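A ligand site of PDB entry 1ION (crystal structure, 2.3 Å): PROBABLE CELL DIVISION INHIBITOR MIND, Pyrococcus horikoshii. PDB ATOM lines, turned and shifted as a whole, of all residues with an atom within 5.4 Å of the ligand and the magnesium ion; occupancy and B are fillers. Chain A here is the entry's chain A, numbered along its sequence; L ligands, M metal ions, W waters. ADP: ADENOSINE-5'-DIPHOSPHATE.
The magnesium ion is bound by an oxygen (O3B) of the ligand (2.1 Å), water W3 (2.2 Å), water W1 (2.2 Å), the side-chain hydroxyl of Thr 17 (2.3 Å) and water W5 (2.3 Å).
O3B of the ligand lies close to N of Thr 17, 3.0 Å away. N of Thr 18 lies within hydrogen-bond range of O2A of the ligand, 3.2 Å away. O2A of the ligand sits at hydrogen-bond distance from OG1 of Thr 18 (2.6 Å). N of Lys 16 lies within hydrogen-bond range of O2B of the ligand (2.9 Å). The side-chain amino group (NZ) of Lys 16 lies within salt-bridge range of an oxygen (O2B) of the ligand. A nitrogen (N6) of the ligand is in hydrogen-bond range of the backbone carbonyl oxygen (O) of Pro 198, at 2.8 Å. N1 of the ligand is in hydrogen-bond range of N of Asp 200. The side-chain amide nitrogen (ND2) of Asn 171 lies within hydrogen-bond range of a nitrogen (N7) of the ligand, at 2.8 Å. O2B of the ligand sits at hydrogen-bond distance from N of Gly 15. O3' of the ligand lies close to NE of Arg 204, 3.3 Å away. O4' of the ligand lies within hydrogen-bond range of NH2 of Arg 172 (2.9 Å). An oxygen (O1B) of the ligand is in hydrogen-bond range of the backbone NH of Gly 13, 3.0 Å away. An oxygen (O2') of the ligand is in hydrogen-bond range of the side-chain hydroxyl of Thr 207. The backbone NH (N) of Thr 14 is in hydrogen-bond range of an oxygen (O2B) of the ligand (3.1 Å).
O of Lys 11 lies within hydrogen-bond range of NZ of Lys 16. The side-chain hydroxyl (OG) of Ser 9 sits at hydrogen-bond distance from the side-chain amino group (NZ) of Lys 16, 3.1 Å away. The side-chain amide nitrogen (ND2) of Asn 171 lies within hydrogen-bond range of the backbone carbonyl oxygen (O) of Thr 14. O of Gly 13 lies within hydrogen-bond range of NH2 of Arg 172, 3.3 Å away. The guanidinium group of Arg 172 lies within salt-bridge range of the side-chain carboxylate of Glu 199, 3.1 Å away. The backbone carbonyl oxygen (O) of Ile 197 sits at hydrogen-bond distance from the backbone NH (N) of Arg 172. The side-chain hydroxyl (OG1) of Thr 14 is in hydrogen-bond range of the backbone carbonyl oxygen (O) of Lys 11, at 3.2 Å. The side-chain hydroxyl of Ser 9 sits at hydrogen-bond distance from the side-chain hydroxyl of Thr 14 (3.1 Å).
The nearest printed residue that does not touch the magnesium ion is Asp 40 (4.1 Å).
Residues that only touch the ligand: Ile 203, Glu 199 and Ile 197. Of the 24 residues printed, 15 come within 4 Å of the ligand. Along chain A the residues within 4 Å of the ligand span positions 13 to 207.
Water W5 lies within hydrogen-bond range of OD1 of Asp 118 (2.6 Å) and O of Cys 119 (2.8 Å). Water W3 bridges O1A of the ligand (2.5 Å) and OD1 of Asn 45 (2.8 Å). Water W4 lies within hydrogen-bond range of an oxygen (O1A) of the ligand and the side-chain amide oxygen of Asn 45. Water W2 lies within hydrogen-bond range of NZ of Lys 16 (2.9 Å) and O1B of the ligand (3.3 Å).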
ATOM      1  N   SER A   9     -12.292   4.407  23.821  1.00  0.00           N
ATOM      2  CA  SER A   9     -11.663   3.202  23.259  1.00  0.00           C
ATOM      3  C   SER A   9     -10.537   3.575  22.301  1.00  0.00           C
ATOM      4  O   SER A   9     -10.323   4.753  22.000  1.00  0.00           O
ATOM      5  CB  SER A   9     -12.675   2.345  22.486  1.00  0.00           C
ATOM      6  OG  SER A   9     -12.984   2.977  21.265  1.00  0.00           O
ATOM      7  N   LYS A  11     -10.283   1.911  19.245  1.00  0.00           N
ATOM      8  CA  LYS A  11     -10.816   1.744  17.892  1.00  0.00           C
ATOM      9  C   LYS A  11     -12.294   2.075  17.763  1.00  0.00           C
ATOM     10  O   LYS A  11     -13.006   2.178  18.751  1.00  0.00           O
ATOM     11  CB  LYS A  11     -10.592   0.305  17.413  1.00  0.00           C
ATOM     12  CG  LYS A  11      -9.145  -0.048  17.218  1.00  0.00           C
ATOM     13  CD  LYS A  11      -8.988  -1.469  16.692  1.00  0.00           C
ATOM     14  CE  LYS A  11      -7.518  -1.829  16.518  1.00  0.00           C
ATOM     15  NZ  LYS A  11      -7.355  -3.223  16.018  1.00  0.00           N
ATOM     16  N   GLY A  12     -12.737   2.231  16.518  1.00  0.00           N
ATOM     17  CA  GLY A  12     -14.122   2.539  16.244  1.00  0.00           C
ATOM     18  C   GLY A  12     -14.922   1.248  16.172  1.00  0.00           C
ATOM     19  O   GLY A  12     -14.342   0.176  15.974  1.00  0.00           O
ATOM     20  N   GLY A  13     -16.239   1.339  16.336  1.00  0.00           N
ATOM     21  CA  GLY A  13     -17.078   0.149  16.279  1.00  0.00           C
ATOM     22  C   GLY A  13     -16.966  -0.788  17.486  1.00  0.00           C
ATOM     23  O   GLY A  13     -17.458  -1.914  17.453  1.00  0.00           O
ATOM     24  N   THR A  14     -16.322  -0.347  18.561  1.00  0.00           N
ATOM     25  CA  THR A  14     -16.183  -1.214  19.719  1.00  0.00           C
ATOM     26  C   THR A  14     -17.363  -1.167  20.702  1.00  0.00           C
ATOM     27  O   THR A  14     -17.464  -2.045  21.566  1.00  0.00           O
ATOM     28  CB  THR A  14     -14.848  -0.968  20.450  1.00  0.00           C
ATOM     29  OG1 THR A  14     -14.717   0.427  20.766  1.00  0.00           O
ATOM     30  CG2 THR A  14     -13.678  -1.408  19.558  1.00  0.00           C
ATOM     31  N   GLY A  15     -18.232  -0.172  20.557  1.00  0.00           N
ATOM     32  CA  GLY A  15     -19.407  -0.073  21.416  1.00  0.00           C
ATOM     33  C   GLY A  15     -19.513   1.118  22.352  1.00  0.00           C
ATOM     34  O   GLY A  15     -20.304   1.087  23.306  1.00  0.00           O
ATOM     35  N   LYS A  16     -18.759   2.179  22.087  1.00  0.00           N
ATOM     36  CA  LYS A  16     -18.775   3.364  22.936  1.00  0.00           C
ATOM     37  C   LYS A  16     -20.168   3.965  23.040  1.00  0.00           C
ATOM     38  O   LYS A  16     -20.655   4.276  24.138  1.00  0.00           O
ATOM     39  CB  LYS A  16     -17.776   4.398  22.417  1.00  0.00           C
ATOM     40  CG  LYS A  16     -16.328   3.940  22.493  1.00  0.00           C
ATOM     41  CD  LYS A  16     -15.374   4.986  21.931  1.00  0.00           C
ATOM     42  CE  LYS A  16     -15.616   5.223  20.454  1.00  0.00           C
ATOM     43  NZ  LYS A  16     -15.422   3.974  19.666  1.00  0.00           N
ATOM     44  N   THR A  17     -20.833   4.126  21.902  1.00  0.00           N
ATOM     45  CA  THR A  17     -22.182   4.690  21.885  1.00  0.00           C
ATOM     46  C   THR A  17     -23.188   3.738  22.537  1.00  0.00           C
ATOM     47  O   THR A  17     -24.090   4.169  23.251  1.00  0.00           O
ATOM     48  CB  THR A  17     -22.620   5.039  20.444  1.00  0.00           C
ATOM     49  OG1 THR A  17     -21.731   6.019  19.917  1.00  0.00           O
ATOM     50  CG2 THR A  17     -24.077   5.593  20.410  1.00  0.00           C
ATOM     51  N   THR A  18     -23.037   2.439  22.293  1.00  0.00           N
ATOM     52  CA  THR A  18     -23.934   1.433  22.871  1.00  0.00           C
ATOM     53  C   THR A  18     -23.806   1.437  24.394  1.00  0.00           C
ATOM     54  O   THR A  18     -24.808   1.429  25.119  1.00  0.00           O
ATOM     55  CB  THR A  18     -23.596   0.016  22.341  1.00  0.00           C
ATOM     56  OG1 THR A  18     -23.714  -0.001  20.915  1.00  0.00           O
ATOM     57  CG2 THR A  18     -24.527  -1.025  22.960  1.00  0.00           C
ATOM     58  N   VAL A  19     -22.575   1.462  24.862  1.00  0.00           N
ATOM     59  CA  VAL A  19     -22.316   1.502  26.287  1.00  0.00           C
ATOM     60  C   VAL A  19     -22.894   2.780  26.891  1.00  0.00           C
ATOM     61  O   VAL A  19     -23.579   2.726  27.925  1.00  0.00           O
ATOM     62  CB  VAL A  19     -20.795   1.426  26.603  1.00  0.00           C
ATOM     63  CG1 VAL A  19     -20.560   1.728  28.116  1.00  0.00           C
ATOM     64  CG2 VAL A  19     -20.276   0.029  26.273  1.00  0.00           C
ATOM     65  N   ASP A  40     -19.088  13.001  20.200  1.00  0.00           N
ATOM     66  CA  ASP A  40     -18.550  12.616  18.897  1.00  0.00           C
ATOM     67  C   ASP A  40     -19.005  13.654  17.867  1.00  0.00           C
ATOM     68  O   ASP A  40     -19.973  13.433  17.133  1.00  0.00           O
ATOM     69  CB  ASP A  40     -19.039  11.241  18.471  1.00  0.00           C
ATOM     70  CG  ASP A  40     -18.227  10.652  17.335  1.00  0.00           C
ATOM     71  OD1 ASP A  40     -17.647  11.427  16.529  1.00  0.00           O
ATOM     72  OD2 ASP A  40     -18.176   9.418  17.223  1.00  0.00           O
ATOM     73  N   ASN A  45     -24.145  10.389  16.943  1.00  0.00           N
ATOM     74  CA  ASN A  45     -24.995   9.214  16.864  1.00  0.00           C
ATOM     75  C   ASN A  45     -25.897   8.981  18.090  1.00  0.00           C
ATOM     76  O   ASN A  45     -26.930   8.309  17.992  1.00  0.00           O
ATOM     77  CB  ASN A  45     -24.074   8.000  16.667  1.00  0.00           C
ATOM     78  CG  ASN A  45     -24.830   6.752  16.352  1.00  0.00           C
ATOM     79  OD1 ASN A  45     -24.505   5.681  16.859  1.00  0.00           O
ATOM     80  ND2 ASN A  45     -25.849   6.862  15.497  1.00  0.00           N
ATOM     81  N   ASP A 118     -20.027  10.243  25.459  1.00  0.00           N
ATOM     82  CA  ASP A 118     -19.828   9.296  24.354  1.00  0.00           C
ATOM     83  C   ASP A 118     -18.707   9.930  23.529  1.00  0.00           C
ATOM     84  O   ASP A 118     -18.886  10.980  22.925  1.00  0.00           O
ATOM     85  CB  ASP A 118     -21.111   9.169  23.529  1.00  0.00           C
ATOM     86  CG  ASP A 118     -21.007   8.111  22.434  1.00  0.00           C
ATOM     87  OD1 ASP A 118     -20.073   7.288  22.458  1.00  0.00           O
ATOM     88  OD2 ASP A 118     -21.890   8.095  21.546  1.00  0.00           O
ATOM     89  N   CYS A 119     -17.536   9.299  23.518  1.00  0.00           N
ATOM     90  CA  CYS A 119     -16.399   9.877  22.804  1.00  0.00           C
ATOM     91  C   CYS A 119     -16.071   9.216  21.467  1.00  0.00           C
ATOM     92  O   CYS A 119     -16.461   8.080  21.218  1.00  0.00           O
ATOM     93  CB  CYS A 119     -15.156   9.809  23.694  1.00  0.00           C
ATOM     94  SG  CYS A 119     -15.282  10.665  25.294  1.00  0.00           S
ATOM     95  N   ASN A 171     -16.484  -5.866  25.501  1.00  0.00           N
ATOM     96  CA  ASN A 171     -17.712  -5.924  24.695  1.00  0.00           C
ATOM     97  C   ASN A 171     -17.570  -6.796  23.447  1.00  0.00           C
ATOM     98  O   ASN A 171     -16.458  -7.066  22.987  1.00  0.00           O
ATOM     99  CB  ASN A 171     -18.127  -4.499  24.296  1.00  0.00           C
ATOM    100  CG  ASN A 171     -19.523  -4.445  23.669  1.00  0.00           C
ATOM    101  OD1 ASN A 171     -20.438  -5.163  24.082  1.00  0.00           O
ATOM    102  ND2 ASN A 171     -19.707  -3.574  22.677  1.00  0.00           N
ATOM    103  N   ARG A 172     -18.702  -7.220  22.918  1.00  0.00           N
ATOM    104  CA  ARG A 172     -18.755  -8.030  21.709  1.00  0.00           C
ATOM    105  C   ARG A 172     -18.124  -9.392  21.948  1.00  0.00           C
ATOM    106  O   ARG A 172     -17.572  -9.981  21.036  1.00  0.00           O
ATOM    107  CB  ARG A 172     -18.020  -7.315  20.570  1.00  0.00           C
ATOM    108  CG  ARG A 172     -18.563  -5.942  20.211  1.00  0.00           C
ATOM    109  CD  ARG A 172     -19.558  -6.037  19.076  1.00  0.00           C
ATOM    110  NE  ARG A 172     -19.303  -4.999  18.085  1.00  0.00           N
ATOM    111  CZ  ARG A 172     -19.852  -4.962  16.868  1.00  0.00           C
ATOM    112  NH1 ARG A 172     -20.697  -5.909  16.497  1.00  0.00           N
ATOM    113  NH2 ARG A 172     -19.543  -3.972  16.039  1.00  0.00           N
ATOM    114  N   ILE A 197     -19.710  -8.099  28.125  1.00  0.00           N
ATOM    115  CA  ILE A 197     -20.985  -7.970  27.432  1.00  0.00           C
ATOM    116  C   ILE A 197     -20.863  -8.816  26.175  1.00  0.00           C
ATOM    117  O   ILE A 197     -19.979  -8.576  25.333  1.00  0.00           O
ATOM    118  CB  ILE A 197     -21.269  -6.485  27.082  1.00  0.00           C
ATOM    119  CG1 ILE A 197     -21.459  -5.702  28.396  1.00  0.00           C
ATOM    120  CG2 ILE A 197     -22.519  -6.382  26.183  1.00  0.00           C
ATOM    121  CD1 ILE A 197     -21.343  -4.245  28.241  1.00  0.00           C
ATOM    122  N   PRO A 198     -21.731  -9.824  26.033  1.00  0.00           N
ATOM    123  CA  PRO A 198     -21.720 -10.731  24.884  1.00  0.00           C
ATOM    124  C   PRO A 198     -22.185 -10.103  23.590  1.00  0.00           C
ATOM    125  O   PRO A 198     -22.918  -9.111  23.588  1.00  0.00           O
ATOM    126  CB  PRO A 198     -22.670 -11.845  25.296  1.00  0.00           C
ATOM    127  CG  PRO A 198     -22.719 -11.743  26.789  1.00  0.00           C
ATOM    128  CD  PRO A 198     -22.738 -10.264  27.014  1.00  0.00           C
ATOM    129  N   GLU A 199     -21.719 -10.673  22.476  1.00  0.00           N
ATOM    130  CA  GLU A 199     -22.177 -10.223  21.188  1.00  0.00           C
ATOM    131  C   GLU A 199     -23.629 -10.714  21.323  1.00  0.00           C
ATOM    132  O   GLU A 199     -23.863 -11.887  21.637  1.00  0.00           O
ATOM    133  CB  GLU A 199     -21.454 -10.965  20.077  1.00  0.00           C
ATOM    134  CG  GLU A 199     -21.889 -10.547  18.681  1.00  0.00           C
ATOM    135  CD  GLU A 199     -21.571  -9.081  18.393  1.00  0.00           C
ATOM    136  OE1 GLU A 199     -20.868  -8.461  19.226  1.00  0.00           O
ATOM    137  OE2 GLU A 199     -22.020  -8.555  17.347  1.00  0.00           O
ATOM    138  N   ASP A 200     -24.581  -9.810  21.131  1.00  0.00           N
ATOM    139  CA  ASP A 200     -25.980 -10.147  21.279  1.00  0.00           C
ATOM    140  C   ASP A 200     -26.859  -9.343  20.305  1.00  0.00           C
ATOM    141  O   ASP A 200     -26.934  -8.125  20.401  1.00  0.00           O
ATOM    142  CB  ASP A 200     -26.418  -9.861  22.714  1.00  0.00           C
ATOM    143  CG  ASP A 200     -27.833 -10.294  22.990  1.00  0.00           C
ATOM    144  OD1 ASP A 200     -28.578 -10.560  22.019  1.00  0.00           O
ATOM    145  OD2 ASP A 200     -28.210 -10.348  24.173  1.00  0.00           O
ATOM    146  N   PRO A 201     -27.544 -10.026  19.373  1.00  0.00           N
ATOM    147  CA  PRO A 201     -28.418  -9.385  18.389  1.00  0.00           C
ATOM    148  C   PRO A 201     -29.433  -8.442  19.044  1.00  0.00           C
ATOM    149  O   PRO A 201     -29.837  -7.443  18.443  1.00  0.00           O
ATOM    150  CB  PRO A 201     -29.077 -10.567  17.690  1.00  0.00           C
ATOM    151  CG  PRO A 201     -27.962 -11.612  17.712  1.00  0.00           C
ATOM    152  CD  PRO A 201     -27.494 -11.488  19.153  1.00  0.00           C
ATOM    153  N   ILE A 203     -28.904  -6.384  21.460  1.00  0.00           N
ATOM    154  CA  ILE A 203     -28.247  -5.100  21.609  1.00  0.00           C
ATOM    155  C   ILE A 203     -28.304  -4.347  20.276  1.00  0.00           C
ATOM    156  O   ILE A 203     -28.549  -3.138  20.248  1.00  0.00           O
ATOM    157  CB  ILE A 203     -26.781  -5.276  22.062  1.00  0.00           C
ATOM    158  CG1 ILE A 203     -26.761  -5.700  23.534  1.00  0.00           C
ATOM    159  CG2 ILE A 203     -25.981  -3.979  21.850  1.00  0.00           C
ATOM    160  CD1 ILE A 203     -25.429  -6.269  23.992  1.00  0.00           C
ATOM    161  N   ARG A 204     -28.101  -5.074  19.179  1.00  0.00           N
ATOM    162  CA  ARG A 204     -28.137  -4.482  17.829  1.00  0.00           C
ATOM    163  C   ARG A 204     -29.544  -4.000  17.480  1.00  0.00           C
ATOM    164  O   ARG A 204     -29.720  -2.954  16.852  1.00  0.00           O
ATOM    165  CB  ARG A 204     -27.674  -5.527  16.783  1.00  0.00           C
ATOM    166  CG  ARG A 204     -27.629  -4.999  15.349  1.00  0.00           C
ATOM    167  CD  ARG A 204     -26.690  -3.793  15.227  1.00  0.00           C
ATOM    168  NE  ARG A 204     -27.183  -2.774  14.297  1.00  0.00           N
ATOM    169  CZ  ARG A 204     -27.130  -2.879  12.966  1.00  0.00           C
ATOM    170  NH1 ARG A 204     -26.620  -3.968  12.395  1.00  0.00           N
ATOM    171  NH2 ARG A 204     -27.598  -1.891  12.206  1.00  0.00           N
ATOM    172  N   THR A 207     -30.166  -0.703  19.199  1.00  0.00           N
ATOM    173  CA  THR A 207     -29.524   0.373  18.455  1.00  0.00           C
ATOM    174  C   THR A 207     -30.458   0.818  17.339  1.00  0.00           C
ATOM    175  O   THR A 207     -30.792   1.994  17.250  1.00  0.00           O
ATOM    176  CB  THR A 207     -28.191  -0.105  17.852  1.00  0.00           C
ATOM    177  OG1 THR A 207     -27.292  -0.421  18.914  1.00  0.00           O
ATOM    178  CG2 THR A 207     -27.549   0.968  16.957  1.00  0.00           C
HETATM  179  PB  ADP L   1     -18.687   2.948  18.522  1.00  0.00           P
HETATM  180  O1B ADP L   1     -18.280   3.340  17.127  1.00  0.00           O
HETATM  181  O2B ADP L   1     -17.532   2.412  19.445  1.00  0.00           O
HETATM  182  O3B ADP L   1     -19.483   4.060  19.245  1.00  0.00           O
HETATM  183  PA  ADP L   1     -21.270   1.651  18.480  1.00  0.00           P
HETATM  184  O1A ADP L   1     -21.800   2.969  18.012  1.00  0.00           O
HETATM  185  O2A ADP L   1     -21.696   1.116  19.751  1.00  0.00           O
HETATM  186  O3A ADP L   1     -19.631   1.721  18.428  1.00  0.00           O
HETATM  187  O5' ADP L   1     -21.567   0.757  17.291  1.00  0.00           O
HETATM  188  C5' ADP L   1     -21.227  -0.570  17.312  1.00  0.00           C
HETATM  189  C4' ADP L   1     -22.164  -1.326  16.431  1.00  0.00           C
HETATM  190  O4' ADP L   1     -21.982  -2.670  16.947  1.00  0.00           O
HETATM  191  C3' ADP L   1     -23.713  -1.064  16.551  1.00  0.00           C
HETATM  192  O3' ADP L   1     -24.340  -1.542  15.340  1.00  0.00           O
HETATM  193  C2' ADP L   1     -24.230  -2.004  17.761  1.00  0.00           C
HETATM  194  O2' ADP L   1     -25.571  -2.495  17.570  1.00  0.00           O
HETATM  195  C1' ADP L   1     -23.086  -3.066  17.664  1.00  0.00           C
HETATM  196  N9  ADP L   1     -22.752  -3.743  18.945  1.00  0.00           N
HETATM  197  C8  ADP L   1     -21.954  -3.226  19.882  1.00  0.00           C
HETATM  198  N7  ADP L   1     -21.858  -3.953  20.907  1.00  0.00           N
HETATM  199  C5  ADP L   1     -22.672  -5.060  20.633  1.00  0.00           C
HETATM  200  C6  ADP L   1     -23.004  -6.273  21.350  1.00  0.00           C
HETATM  201  N6  ADP L   1     -22.483  -6.571  22.598  1.00  0.00           N
HETATM  202  N1  ADP L   1     -23.871  -7.169  20.746  1.00  0.00           N
HETATM  203  C2  ADP L   1     -24.368  -6.879  19.537  1.00  0.00           C
HETATM  204  N3  ADP L   1     -24.105  -5.765  18.806  1.00  0.00           N
HETATM  205  C4  ADP L   1     -23.249  -4.912  19.414  1.00  0.00           C
HETATM  206 MG    MG M   1     -19.968   5.969  18.442  1.00  0.00          MG
HETATM  207  O   HOH W   1     -20.751   7.990  17.930  1.00  0.00           O
HETATM  208  O   HOH W   2     -15.692   5.371  17.089  1.00  0.00           O
HETATM  209  O   HOH W   3     -21.724   5.334  17.252  1.00  0.00           O
HETATM  210  O   HOH W   4     -24.657   2.662  18.178  1.00  0.00           O
HETATM  211  O   HOH W   5     -18.890   7.168  20.108  1.00  0.00           O
